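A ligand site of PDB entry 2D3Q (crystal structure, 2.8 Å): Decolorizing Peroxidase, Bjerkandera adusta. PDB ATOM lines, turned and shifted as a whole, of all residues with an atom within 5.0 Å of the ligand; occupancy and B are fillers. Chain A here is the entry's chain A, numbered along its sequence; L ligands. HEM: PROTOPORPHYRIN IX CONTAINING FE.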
ATOM      1  N   GLU A 165     -18.782  12.190  30.454  1.00  0.00           N
ATOM      2  CA  GLU A 165     -20.181  11.812  30.319  1.00  0.00           C
ATOM      3  C   GLU A 165     -20.778  12.060  31.712  1.00  0.00           C
ATOM      4  O   GLU A 165     -20.052  12.452  32.630  1.00  0.00           O
ATOM      5  CB  GLU A 165     -20.302  10.354  29.880  1.00  0.00           C
ATOM      6  CG  GLU A 165     -19.443   9.403  30.651  1.00  0.00           C
ATOM      7  CD  GLU A 165     -19.994   9.146  32.025  1.00  0.00           C
ATOM      8  OE1 GLU A 165     -19.227   9.313  33.005  1.00  0.00           O
ATOM      9  OE2 GLU A 165     -21.188   8.789  32.123  1.00  0.00           O
ATOM     10  N   PHE A 167     -21.678  10.229  34.305  1.00  0.00           N
ATOM     11  CA  PHE A 167     -21.248   9.529  35.517  1.00  0.00           C
ATOM     12  C   PHE A 167     -19.950  10.191  35.973  1.00  0.00           C
ATOM     13  O   PHE A 167     -19.402   9.868  37.022  1.00  0.00           O
ATOM     14  CB  PHE A 167     -20.999   8.028  35.265  1.00  0.00           C
ATOM     15  CG  PHE A 167     -22.245   7.231  35.067  1.00  0.00           C
ATOM     16  CD1 PHE A 167     -23.411   7.562  35.746  1.00  0.00           C
ATOM     17  CD2 PHE A 167     -22.258   6.157  34.191  1.00  0.00           C
ATOM     18  CE1 PHE A 167     -24.575   6.829  35.562  1.00  0.00           C
ATOM     19  CE2 PHE A 167     -23.417   5.412  34.002  1.00  0.00           C
ATOM     20  CZ  PHE A 167     -24.574   5.746  34.684  1.00  0.00           C
ATOM     21  N   PHE A 169     -17.012  10.392  33.997  1.00  0.00           N
ATOM     22  CA  PHE A 169     -15.816   9.896  33.324  1.00  0.00           C
ATOM     23  C   PHE A 169     -15.511  10.549  31.975  1.00  0.00           C
ATOM     24  O   PHE A 169     -16.408  10.719  31.153  1.00  0.00           O
ATOM     25  CB  PHE A 169     -15.926   8.400  33.105  1.00  0.00           C
ATOM     26  CG  PHE A 169     -15.925   7.619  34.375  1.00  0.00           C
ATOM     27  CD1 PHE A 169     -14.797   6.909  34.777  1.00  0.00           C
ATOM     28  CD2 PHE A 169     -17.058   7.616  35.198  1.00  0.00           C
ATOM     29  CE1 PHE A 169     -14.787   6.204  35.969  1.00  0.00           C
ATOM     30  CE2 PHE A 169     -17.063   6.919  36.391  1.00  0.00           C
ATOM     31  CZ  PHE A 169     -15.923   6.209  36.787  1.00  0.00           C
ATOM     32  N   LEU A 170     -14.248  10.899  31.767  1.00  0.00           N
ATOM     33  CA  LEU A 170     -13.812  11.500  30.516  1.00  0.00           C
ATOM     34  C   LEU A 170     -14.092  10.519  29.388  1.00  0.00           C
ATOM     35  O   LEU A 170     -13.663   9.358  29.424  1.00  0.00           O
ATOM     36  CB  LEU A 170     -12.311  11.794  30.578  1.00  0.00           C
ATOM     37  CG  LEU A 170     -11.711  12.400  29.319  1.00  0.00           C
ATOM     38  CD1 LEU A 170     -12.272  13.809  29.095  1.00  0.00           C
ATOM     39  CD2 LEU A 170     -10.201  12.437  29.444  1.00  0.00           C
ATOM     40  N   ASP A 171     -14.815  10.974  28.362  1.00  0.00           N
ATOM     41  CA  ASP A 171     -15.163  10.102  27.251  1.00  0.00           C
ATOM     42  C   ASP A 171     -14.540  10.533  25.941  1.00  0.00           C
ATOM     43  O   ASP A 171     -14.261  11.712  25.728  1.00  0.00           O
ATOM     44  CB  ASP A 171     -16.687  10.039  27.086  1.00  0.00           C
ATOM     45  CG  ASP A 171     -17.136   8.851  26.256  1.00  0.00           C
ATOM     46  OD1 ASP A 171     -16.264   8.072  25.820  1.00  0.00           O
ATOM     47  OD2 ASP A 171     -18.372   8.692  26.036  1.00  0.00           O
ATOM     48  N   GLY A 172     -14.308   9.560  25.066  1.00  0.00           N
ATOM     49  CA  GLY A 172     -13.732   9.853  23.766  1.00  0.00           C
ATOM     50  C   GLY A 172     -12.229   9.743  23.676  1.00  0.00           C
ATOM     51  O   GLY A 172     -11.623  10.306  22.777  1.00  0.00           O
ATOM     52  N   ILE A 173     -11.616   9.004  24.604  1.00  0.00           N
ATOM     53  CA  ILE A 173     -10.169   8.849  24.606  1.00  0.00           C
ATOM     54  C   ILE A 173      -9.647   7.880  23.538  1.00  0.00           C
ATOM     55  O   ILE A 173      -8.841   8.258  22.697  1.00  0.00           O
ATOM     56  CB  ILE A 173      -9.688   8.402  25.990  1.00  0.00           C
ATOM     57  CG1 ILE A 173     -10.126   9.424  27.030  1.00  0.00           C
ATOM     58  CG2 ILE A 173      -8.161   8.234  25.994  1.00  0.00           C
ATOM     59  CD1 ILE A 173      -9.829   9.034  28.457  1.00  0.00           C
ATOM     60  N   SER A 174     -10.112   6.631  23.570  1.00  0.00           N
ATOM     61  CA  SER A 174      -9.653   5.612  22.630  1.00  0.00           C
ATOM     62  C   SER A 174     -10.535   5.412  21.376  1.00  0.00           C
ATOM     63  O   SER A 174     -11.715   5.059  21.454  1.00  0.00           O
ATOM     64  CB  SER A 174      -9.524   4.295  23.391  1.00  0.00           C
ATOM     65  OG  SER A 174      -8.862   3.320  22.602  1.00  0.00           O
ATOM     66  N   GLN A 175      -9.929   5.637  20.212  1.00  0.00           N
ATOM     67  CA  GLN A 175     -10.630   5.519  18.933  1.00  0.00           C
ATOM     68  C   GLN A 175      -9.760   4.867  17.866  1.00  0.00           C
ATOM     69  O   GLN A 175      -8.572   5.164  17.747  1.00  0.00           O
ATOM     70  CB  GLN A 175     -11.024   6.906  18.423  1.00  0.00           C
ATOM     71  CG  GLN A 175     -11.962   7.658  19.324  1.00  0.00           C
ATOM     72  CD  GLN A 175     -13.408   7.328  19.066  1.00  0.00           C
ATOM     73  OE1 GLN A 175     -13.740   6.217  18.632  1.00  0.00           O
ATOM     74  NE2 GLN A 175     -14.281   8.285  19.338  1.00  0.00           N
ATOM     75  N   PHE A 223     -29.546   6.703  25.535  1.00  0.00           N
ATOM     76  CA  PHE A 223     -29.358   6.182  26.886  1.00  0.00           C
ATOM     77  C   PHE A 223     -29.711   7.173  27.998  1.00  0.00           C
ATOM     78  O   PHE A 223     -29.285   8.326  27.960  1.00  0.00           O
ATOM     79  CB  PHE A 223     -27.901   5.760  27.120  1.00  0.00           C
ATOM     80  CG  PHE A 223     -27.448   4.563  26.329  1.00  0.00           C
ATOM     81  CD1 PHE A 223     -28.249   3.436  26.234  1.00  0.00           C
ATOM     82  CD2 PHE A 223     -26.184   4.555  25.738  1.00  0.00           C
ATOM     83  CE1 PHE A 223     -27.787   2.300  25.546  1.00  0.00           C
ATOM     84  CE2 PHE A 223     -25.723   3.415  25.064  1.00  0.00           C
ATOM     85  CZ  PHE A 223     -26.534   2.284  24.966  1.00  0.00           C
ATOM     86  N   GLN A 225     -29.174   7.976  31.909  1.00  0.00           N
ATOM     87  CA  GLN A 225     -28.303   7.561  32.998  1.00  0.00           C
ATOM     88  C   GLN A 225     -28.807   7.906  34.394  1.00  0.00           C
ATOM     89  O   GLN A 225     -29.253   9.033  34.660  1.00  0.00           O
ATOM     90  CB  GLN A 225     -26.901   8.140  32.797  1.00  0.00           C
ATOM     91  CG  GLN A 225     -26.286   7.804  31.428  1.00  0.00           C
ATOM     92  CD  GLN A 225     -24.894   8.375  31.239  1.00  0.00           C
ATOM     93  OE1 GLN A 225     -23.925   7.907  31.853  1.00  0.00           O
ATOM     94  NE2 GLN A 225     -24.773   9.383  30.378  1.00  0.00           N
ATOM     95  N   PHE A 261     -15.118   0.851  35.093  1.00  0.00           N
ATOM     96  CA  PHE A 261     -14.882   1.397  33.754  1.00  0.00           C
ATOM     97  C   PHE A 261     -13.560   0.999  33.132  1.00  0.00           C
ATOM     98  O   PHE A 261     -13.504   0.714  31.931  1.00  0.00           O
ATOM     99  CB  PHE A 261     -14.969   2.930  33.798  1.00  0.00           C
ATOM    100  CG  PHE A 261     -16.338   3.465  33.511  1.00  0.00           C
ATOM    101  CD1 PHE A 261     -16.790   3.596  32.202  1.00  0.00           C
ATOM    102  CD2 PHE A 261     -17.177   3.858  34.545  1.00  0.00           C
ATOM    103  CE1 PHE A 261     -18.048   4.120  31.928  1.00  0.00           C
ATOM    104  CE2 PHE A 261     -18.433   4.374  34.277  1.00  0.00           C
ATOM    105  CZ  PHE A 261     -18.867   4.512  32.971  1.00  0.00           C
ATOM    106  N   ARG A 263     -11.016   2.980  33.709  1.00  0.00           N
ATOM    107  CA  ARG A 263     -10.373   4.297  33.691  1.00  0.00           C
ATOM    108  C   ARG A 263     -10.858   5.112  34.867  1.00  0.00           C
ATOM    109  O   ARG A 263     -11.981   4.924  35.358  1.00  0.00           O
ATOM    110  CB  ARG A 263     -10.718   5.072  32.408  1.00  0.00           C
ATOM    111  CG  ARG A 263      -9.958   4.620  31.183  1.00  0.00           C
ATOM    112  CD  ARG A 263     -10.193   5.551  29.975  1.00  0.00           C
ATOM    113  NE  ARG A 263      -9.690   4.945  28.745  1.00  0.00           N
ATOM    114  CZ  ARG A 263      -8.436   5.046  28.310  1.00  0.00           C
ATOM    115  NH1 ARG A 263      -7.540   5.745  29.001  1.00  0.00           N
ATOM    116  NH2 ARG A 263      -8.063   4.402  27.199  1.00  0.00           N
ATOM    117  N   ASN A 289      -3.355   6.110  26.663  1.00  0.00           N
ATOM    118  CA  ASN A 289      -3.937   4.965  25.973  1.00  0.00           C
ATOM    119  C   ASN A 289      -2.914   3.906  25.596  1.00  0.00           C
ATOM    120  O   ASN A 289      -3.208   2.981  24.845  1.00  0.00           O
ATOM    121  CB  ASN A 289      -4.685   5.458  24.733  1.00  0.00           C
ATOM    122  CG  ASN A 289      -5.723   4.460  24.228  1.00  0.00           C
ATOM    123  OD1 ASN A 289      -6.507   3.907  25.019  1.00  0.00           O
ATOM    124  ND2 ASN A 289      -5.747   4.246  22.917  1.00  0.00           N
ATOM    125  N   PHE A 291      -1.539   0.990  26.629  1.00  0.00           N
ATOM    126  CA  PHE A 291      -1.629  -0.199  27.468  1.00  0.00           C
ATOM    127  C   PHE A 291      -2.409  -1.261  26.685  1.00  0.00           C
ATOM    128  O   PHE A 291      -3.076  -0.926  25.712  1.00  0.00           O
ATOM    129  CB  PHE A 291      -2.391   0.149  28.740  1.00  0.00           C
ATOM    130  CG  PHE A 291      -3.812   0.545  28.485  1.00  0.00           C
ATOM    131  CD1 PHE A 291      -4.818  -0.413  28.430  1.00  0.00           C
ATOM    132  CD2 PHE A 291      -4.138   1.885  28.256  1.00  0.00           C
ATOM    133  CE1 PHE A 291      -6.138  -0.038  28.154  1.00  0.00           C
ATOM    134  CE2 PHE A 291      -5.449   2.264  27.981  1.00  0.00           C
ATOM    135  CZ  PHE A 291      -6.444   1.301  27.934  1.00  0.00           C
ATOM    136  N   HIS A 308     -15.749  -1.965  31.626  1.00  0.00           N
ATOM    137  CA  HIS A 308     -16.306  -1.425  30.380  1.00  0.00           C
ATOM    138  C   HIS A 308     -15.335  -1.398  29.193  1.00  0.00           C
ATOM    139  O   HIS A 308     -15.560  -2.076  28.180  1.00  0.00           O
ATOM    140  CB  HIS A 308     -16.844  -0.014  30.608  1.00  0.00           C
ATOM    141  CG  HIS A 308     -17.581   0.542  29.413  1.00  0.00           C
ATOM    142  ND1 HIS A 308     -18.724  -0.044  28.913  1.00  0.00           N
ATOM    143  CD2 HIS A 308     -17.311   1.606  28.621  1.00  0.00           C
ATOM    144  CE1 HIS A 308     -19.128   0.644  27.857  1.00  0.00           C
ATOM    145  NE2 HIS A 308     -18.294   1.650  27.659  1.00  0.00           N
ATOM    146  N   VAL A 309     -14.268  -0.634  29.313  1.00  0.00           N
ATOM    147  CA  VAL A 309     -13.303  -0.504  28.228  1.00  0.00           C
ATOM    148  C   VAL A 309     -12.644  -1.825  27.830  1.00  0.00           C
ATOM    149  O   VAL A 309     -12.335  -2.047  26.663  1.00  0.00           O
ATOM    150  CB  VAL A 309     -12.203   0.537  28.572  1.00  0.00           C
ATOM    151  CG1 VAL A 309     -12.844   1.897  28.865  1.00  0.00           C
ATOM    152  CG2 VAL A 309     -11.394   0.055  29.761  1.00  0.00           C
ATOM    153  N   THR A 312     -15.373  -3.769  25.775  1.00  0.00           N
ATOM    154  CA  THR A 312     -15.639  -3.200  24.442  1.00  0.00           C
ATOM    155  C   THR A 312     -14.380  -3.234  23.557  1.00  0.00           C
ATOM    156  O   THR A 312     -14.477  -3.161  22.330  1.00  0.00           O
ATOM    157  CB  THR A 312     -16.142  -1.754  24.550  1.00  0.00           C
ATOM    158  OG1 THR A 312     -15.088  -0.909  25.049  1.00  0.00           O
ATOM    159  CG2 THR A 312     -17.317  -1.682  25.485  1.00  0.00           C
ATOM    160  N   ASN A 313     -13.212  -3.316  24.176  1.00  0.00           N
ATOM    161  CA  ASN A 313     -11.945  -3.425  23.445  1.00  0.00           C
ATOM    162  C   ASN A 313     -10.971  -4.178  24.345  1.00  0.00           C
ATOM    163  O   ASN A 313     -10.170  -3.586  25.060  1.00  0.00           O
ATOM    164  CB  ASN A 313     -11.372  -2.051  23.082  1.00  0.00           C
ATOM    165  CG  ASN A 313     -10.033  -2.151  22.353  1.00  0.00           C
ATOM    166  OD1 ASN A 313      -9.634  -3.215  21.888  1.00  0.00           O
ATOM    167  ND2 ASN A 313      -9.340  -1.026  22.244  1.00  0.00           N
ATOM    168  N   ARG A 315      -8.387  -5.667  23.720  1.00  0.00           N
ATOM    169  CA  ARG A 315      -6.999  -5.529  23.308  1.00  0.00           C
ATOM    170  C   ARG A 315      -6.290  -6.880  23.294  1.00  0.00           C
ATOM    171  O   ARG A 315      -6.631  -7.752  22.513  1.00  0.00           O
ATOM    172  CB  ARG A 315      -6.259  -4.553  24.232  1.00  0.00           C
ATOM    173  CG  ARG A 315      -7.033  -3.264  24.459  1.00  0.00           C
ATOM    174  CD  ARG A 315      -6.152  -2.076  24.792  1.00  0.00           C
ATOM    175  NE  ARG A 315      -6.978  -0.872  24.851  1.00  0.00           N
ATOM    176  CZ  ARG A 315      -6.519   0.367  24.763  1.00  0.00           C
ATOM    177  NH1 ARG A 315      -5.220   0.598  24.600  1.00  0.00           N
ATOM    178  NH2 ARG A 315      -7.361   1.387  24.819  1.00  0.00           N
ATOM    179  N   ARG A 329     -16.637   6.197  17.646  1.00  0.00           N
ATOM    180  CA  ARG A 329     -17.732   6.681  18.481  1.00  0.00           C
ATOM    181  C   ARG A 329     -17.776   8.194  18.363  1.00  0.00           C
ATOM    182  O   ARG A 329     -16.739   8.839  18.223  1.00  0.00           O
ATOM    183  CB  ARG A 329     -17.534   6.255  19.932  1.00  0.00           C
ATOM    184  CG  ARG A 329     -17.934   4.818  20.204  1.00  0.00           C
ATOM    185  CD  ARG A 329     -17.444   4.387  21.572  1.00  0.00           C
ATOM    186  NE  ARG A 329     -16.010   4.625  21.692  1.00  0.00           N
ATOM    187  CZ  ARG A 329     -15.464   5.298  22.691  1.00  0.00           C
ATOM    188  NH1 ARG A 329     -16.223   5.805  23.658  1.00  0.00           N
ATOM    189  NH2 ARG A 329     -14.157   5.493  22.712  1.00  0.00           N
ATOM    190  N   LEU A 354     -26.787   9.791  27.683  1.00  0.00           N
ATOM    191  CA  LEU A 354     -25.893   9.881  26.541  1.00  0.00           C
ATOM    192  C   LEU A 354     -26.596   9.589  25.225  1.00  0.00           C
ATOM    193  O   LEU A 354     -27.433   8.692  25.137  1.00  0.00           O
ATOM    194  CB  LEU A 354     -24.761   8.889  26.713  1.00  0.00           C
ATOM    195  CG  LEU A 354     -23.576   8.920  25.746  1.00  0.00           C
ATOM    196  CD1 LEU A 354     -22.743  10.172  25.984  1.00  0.00           C
ATOM    197  CD2 LEU A 354     -22.742   7.660  25.960  1.00  0.00           C
ATOM    198  N   PHE A 356     -25.690   8.181  22.255  1.00  0.00           N
ATOM    199  CA  PHE A 356     -24.617   7.308  21.766  1.00  0.00           C
ATOM    200  C   PHE A 356     -24.629   7.089  20.252  1.00  0.00           C
ATOM    201  O   PHE A 356     -25.646   6.707  19.659  1.00  0.00           O
ATOM    202  CB  PHE A 356     -24.721   5.960  22.497  1.00  0.00           C
ATOM    203  CG  PHE A 356     -23.665   4.957  22.119  1.00  0.00           C
ATOM    204  CD1 PHE A 356     -22.450   4.919  22.794  1.00  0.00           C
ATOM    205  CD2 PHE A 356     -23.906   4.039  21.105  1.00  0.00           C
ATOM    206  CE1 PHE A 356     -21.488   3.964  22.463  1.00  0.00           C
ATOM    207  CE2 PHE A 356     -22.950   3.076  20.764  1.00  0.00           C
ATOM    208  CZ  PHE A 356     -21.736   3.034  21.452  1.00  0.00           C
ATOM    209  N   GLU A 358     -22.244   5.149  17.248  1.00  0.00           N
ATOM    210  CA  GLU A 358     -21.098   4.307  16.925  1.00  0.00           C
ATOM    211  C   GLU A 358     -21.105   3.923  15.430  1.00  0.00           C
ATOM    212  O   GLU A 358     -22.106   3.445  14.888  1.00  0.00           O
ATOM    213  CB  GLU A 358     -21.092   3.061  17.827  1.00  0.00           C
ATOM    214  CG  GLU A 358     -19.891   2.125  17.626  1.00  0.00           C
ATOM    215  CD  GLU A 358     -19.718   1.126  18.783  1.00  0.00           C
ATOM    216  OE1 GLU A 358     -20.728   0.604  19.296  1.00  0.00           O
ATOM    217  OE2 GLU A 358     -18.554   0.873  19.164  1.00  0.00           O
ATOM    218  N   PHE A 367     -20.525  -2.280  17.281  1.00  0.00           N
ATOM    219  CA  PHE A 367     -21.480  -2.065  18.365  1.00  0.00           C
ATOM    220  C   PHE A 367     -22.163  -3.367  18.803  1.00  0.00           C
ATOM    221  O   PHE A 367     -22.052  -3.773  19.955  1.00  0.00           O
ATOM    222  CB  PHE A 367     -22.556  -1.070  17.922  1.00  0.00           C
ATOM    223  CG  PHE A 367     -23.811  -1.149  18.732  1.00  0.00           C
ATOM    224  CD1 PHE A 367     -23.863  -0.602  20.000  1.00  0.00           C
ATOM    225  CD2 PHE A 367     -24.919  -1.841  18.258  1.00  0.00           C
ATOM    226  CE1 PHE A 367     -25.001  -0.743  20.791  1.00  0.00           C
ATOM    227  CE2 PHE A 367     -26.051  -1.990  19.031  1.00  0.00           C
ATOM    228  CZ  PHE A 367     -26.097  -1.435  20.310  1.00  0.00           C
ATOM    229  N   GLN A 370     -19.622  -5.841  20.342  1.00  0.00           N
ATOM    230  CA  GLN A 370     -19.159  -5.400  21.638  1.00  0.00           C
ATOM    231  C   GLN A 370     -20.277  -5.633  22.654  1.00  0.00           C
ATOM    232  O   GLN A 370     -20.040  -6.109  23.746  1.00  0.00           O
ATOM    233  CB  GLN A 370     -18.800  -3.915  21.573  1.00  0.00           C
ATOM    234  CG  GLN A 370     -17.583  -3.653  20.710  1.00  0.00           C
ATOM    235  CD  GLN A 370     -17.503  -2.222  20.200  1.00  0.00           C
ATOM    236  OE1 GLN A 370     -18.016  -1.294  20.835  1.00  0.00           O
ATOM    237  NE2 GLN A 370     -16.843  -2.037  19.064  1.00  0.00           N
ATOM    238  N   GLN A 371     -21.503  -5.323  22.257  1.00  0.00           N
ATOM    239  CA  GLN A 371     -22.649  -5.496  23.141  1.00  0.00           C
ATOM    240  C   GLN A 371     -23.013  -6.942  23.466  1.00  0.00           C
ATOM    241  O   GLN A 371     -23.000  -7.355  24.630  1.00  0.00           O
ATOM    242  CB  GLN A 371     -23.878  -4.810  22.536  1.00  0.00           C
ATOM    243  CG  GLN A 371     -25.077  -4.883  23.435  1.00  0.00           C
ATOM    244  CD  GLN A 371     -24.829  -4.173  24.745  1.00  0.00           C
ATOM    245  OE1 GLN A 371     -24.618  -2.954  24.780  1.00  0.00           O
ATOM    246  NE2 GLN A 371     -24.844  -4.930  25.834  1.00  0.00           N
ATOM    247  N   ILE A 393     -21.392  -1.469  33.400  1.00  0.00           N
ATOM    248  CA  ILE A 393     -21.995  -0.269  32.824  1.00  0.00           C
ATOM    249  C   ILE A 393     -23.070  -0.465  31.751  1.00  0.00           C
ATOM    250  O   ILE A 393     -24.141   0.132  31.854  1.00  0.00           O
ATOM    251  CB  ILE A 393     -20.923   0.696  32.294  1.00  0.00           C
ATOM    252  CG1 ILE A 393     -20.287   1.477  33.442  1.00  0.00           C
ATOM    253  CG2 ILE A 393     -21.573   1.739  31.399  1.00  0.00           C
ATOM    254  CD1 ILE A 393     -20.025   0.683  34.691  1.00  0.00           C
ATOM    255  N   ILE A 394     -22.794  -1.280  30.739  1.00  0.00           N
ATOM    256  CA  ILE A 394     -23.777  -1.498  29.687  1.00  0.00           C
ATOM    257  C   ILE A 394     -24.182  -2.948  29.438  1.00  0.00           C
ATOM    258  O   ILE A 394     -25.006  -3.217  28.555  1.00  0.00           O
ATOM    259  CB  ILE A 394     -23.311  -0.947  28.331  1.00  0.00           C
ATOM    260  CG1 ILE A 394     -21.998  -1.607  27.919  1.00  0.00           C
ATOM    261  CG2 ILE A 394     -23.172   0.548  28.410  1.00  0.00           C
ATOM    262  CD1 ILE A 394     -21.831  -1.739  26.434  1.00  0.00           C
ATOM    263  N   VAL A 420     -27.691   2.375  33.146  1.00  0.00           N
ATOM    264  CA  VAL A 420     -27.781   2.850  31.772  1.00  0.00           C
ATOM    265  C   VAL A 420     -29.073   2.291  31.202  1.00  0.00           C
ATOM    266  O   VAL A 420     -29.232   1.077  31.068  1.00  0.00           O
ATOM    267  CB  VAL A 420     -26.587   2.365  30.930  1.00  0.00           C
ATOM    268  CG1 VAL A 420     -26.756   2.802  29.485  1.00  0.00           C
ATOM    269  CG2 VAL A 420     -25.294   2.911  31.518  1.00  0.00           C
HETATM  270  CHA HEM L   1     -15.216   3.631  26.016  1.00  0.00           C
HETATM  271  CHB HEM L   1     -18.586   5.341  27.844  1.00  0.00           C
HETATM  272  CHC HEM L   1     -21.645   2.955  26.250  1.00  0.00           C
HETATM  273  CHD HEM L   1     -18.326   1.253  23.768  1.00  0.00           C
HETATM  274  C1A HEM L   1     -15.566   4.600  26.940  1.00  0.00           C
HETATM  275  C2A HEM L   1     -15.021   5.456  27.972  1.00  0.00           C
HETATM  276  C3A HEM L   1     -16.073   5.867  28.740  1.00  0.00           C
HETATM  277  C4A HEM L   1     -17.236   5.245  28.143  1.00  0.00           C
HETATM  278  CMA HEM L   1     -16.478   6.906  29.751  1.00  0.00           C
HETATM  279  CAA HEM L   1     -13.585   5.873  28.220  1.00  0.00           C
HETATM  280  CBA HEM L   1     -12.817   6.423  26.993  1.00  0.00           C
HETATM  281  CGA HEM L   1     -12.141   5.752  25.942  1.00  0.00           C
HETATM  282  O1A HEM L   1     -11.376   4.708  26.193  1.00  0.00           O
HETATM  283  O2A HEM L   1     -12.671   6.568  25.151  1.00  0.00           O
HETATM  284  C1B HEM L   1     -19.896   5.086  28.200  1.00  0.00           C
HETATM  285  C2B HEM L   1     -21.137   5.530  28.822  1.00  0.00           C
HETATM  286  C3B HEM L   1     -22.085   4.786  28.202  1.00  0.00           C
HETATM  287  C4B HEM L   1     -21.427   3.920  27.232  1.00  0.00           C
HETATM  288  CMB HEM L   1     -21.116   6.348  30.077  1.00  0.00           C
HETATM  289  CAB HEM L   1     -23.571   4.801  28.179  1.00  0.00           C
HETATM  290  CBB HEM L   1     -24.474   5.450  29.257  1.00  0.00           C
HETATM  291  C1C HEM L   1     -21.249   2.083  25.287  1.00  0.00           C
HETATM  292  C2C HEM L   1     -21.922   1.125  24.428  1.00  0.00           C
HETATM  293  C3C HEM L   1     -20.860   0.627  23.773  1.00  0.00           C
HETATM  294  C4C HEM L   1     -19.639   1.245  24.208  1.00  0.00           C
HETATM  295  CMC HEM L   1     -23.411   0.869  24.447  1.00  0.00           C
HETATM  296  CAC HEM L   1     -20.846  -0.551  22.804  1.00  0.00           C
HETATM  297  CBC HEM L   1     -21.827  -1.751  22.602  1.00  0.00           C
HETATM  298  C1D HEM L   1     -17.011   1.690  23.879  1.00  0.00           C
HETATM  299  C2D HEM L   1     -15.703   1.620  23.240  1.00  0.00           C
HETATM  300  C3D HEM L   1     -14.696   2.253  23.888  1.00  0.00           C
HETATM  301  C4D HEM L   1     -15.533   2.713  24.997  1.00  0.00           C
HETATM  302  CMD HEM L   1     -15.559   0.793  21.996  1.00  0.00           C
HETATM  303  CAD HEM L   1     -13.211   2.364  23.841  1.00  0.00           C
HETATM  304  CBD HEM L   1     -12.408   1.042  24.211  1.00  0.00           C
HETATM  305  CGD HEM L   1     -11.036   1.202  23.888  1.00  0.00           C
HETATM  306  O1D HEM L   1     -10.272   1.155  24.906  1.00  0.00           O
HETATM  307  O2D HEM L   1     -10.607   1.384  22.710  1.00  0.00           O
HETATM  308  NA  HEM L   1     -16.935   4.469  27.042  1.00  0.00           N
HETATM  309  NB  HEM L   1     -20.052   4.117  27.243  1.00  0.00           N
HETATM  310  NC  HEM L   1     -19.851   2.197  25.182  1.00  0.00           N
HETATM  311  ND  HEM L   1     -16.861   2.427  25.034  1.00  0.00           N
HETATM  312 FE   HEM L   1     -18.387   3.192  26.214  1.00  0.00          FE
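The backbone NH (N) of Leu 354 sits at hydrogen-bond distance from the backbone carbonyl oxygen (O) of Phe 223, 2.9 Å away.
The side-chain hydroxyl (OG1) of Thr 312 is in hydrogen-bond range of the backbone carbonyl oxygen (O) of Val 309, 3.4 Å away.
NH2 of Arg 329 lies within hydrogen-bond range of O of Ser 174, at 2.8 Å.
N of Phe 169 sits at hydrogen-bond distance from OE1 of Glu 165, at 2.7 Å.
The side-chain amide oxygen (OD1) of Asn 289 sits at hydrogen-bond distance from the guanidinium group (NH2) of Arg 263, at 2.7 Å.
The guanidinium group (NH2) of Arg 315 sits at hydrogen-bond distance from the side-chain amide oxygen (OD1) of Asn 289, at 2.7 Å.
The side-chain amide nitrogen of Gln 225 sits close to the backbone NH of Leu 354.
The side-chain carboxylate (OE2) of Glu 358 lies close to the side-chain amide oxygen (OE1) of Gln 370.
Merely in contact with the ligand: Glu 165 (3.2 Å), Phe 169 (3.7 Å), Leu 170 (3.7 Å), Asp 171 (3.6 Å), Phe 223 (3.5 Å), Gln 225 (3.6 Å), Phe 261 (3.9 Å), Val 309 (3.9 Å), Thr 312 (3.2 Å), Leu 354 (3.7 Å), Phe 356 (3.4 Å), Glu 358 (3.7 Å), Phe 367 (3.3 Å), Gln 370 (3.4 Å), Gln 371 (3.6 Å), Ile 394 (3.5 Å) and Val 420 (3.5 Å).
Hydrophobic or aromatic side chains within 4 Å of the ligand: Phe 169, Ile 173, Phe 223, Phe 261, His 308, Leu 354, Phe 356, Phe 367, Ile 394 and Val 420.
NH2 of Arg 329 lies within salt-bridge range of O2A of the ligand.
OG of Ser 174 is in hydrogen-bond range of O2D of the ligand (2.6 Å).
ND2 of Asn 313 sits at hydrogen-bond distance from O2D of the ligand (2.8 Å).
An oxygen (O2A) of the ligand is in hydrogen-bond range of the backbone NH (N) of Ile 173 (2.7 Å).
An iron atom (FE) of the ligand is bound by a ring nitrogen (NE2) of His 308.
An oxygen (O1D) of the ligand is in salt-bridge range of the guanidinium group (NH2) of Arg 315, at 2.9 Å.
The backbone NH of Gly 172 sits at hydrogen-bond distance from an oxygen (O2A) of the ligand, 3.4 Å away.
NE of Arg 263 is in salt-bridge range of O1A of the ligand.
N of Ser 174 sits at hydrogen-bond distance from O2A of the ligand, at 3.0 Å.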
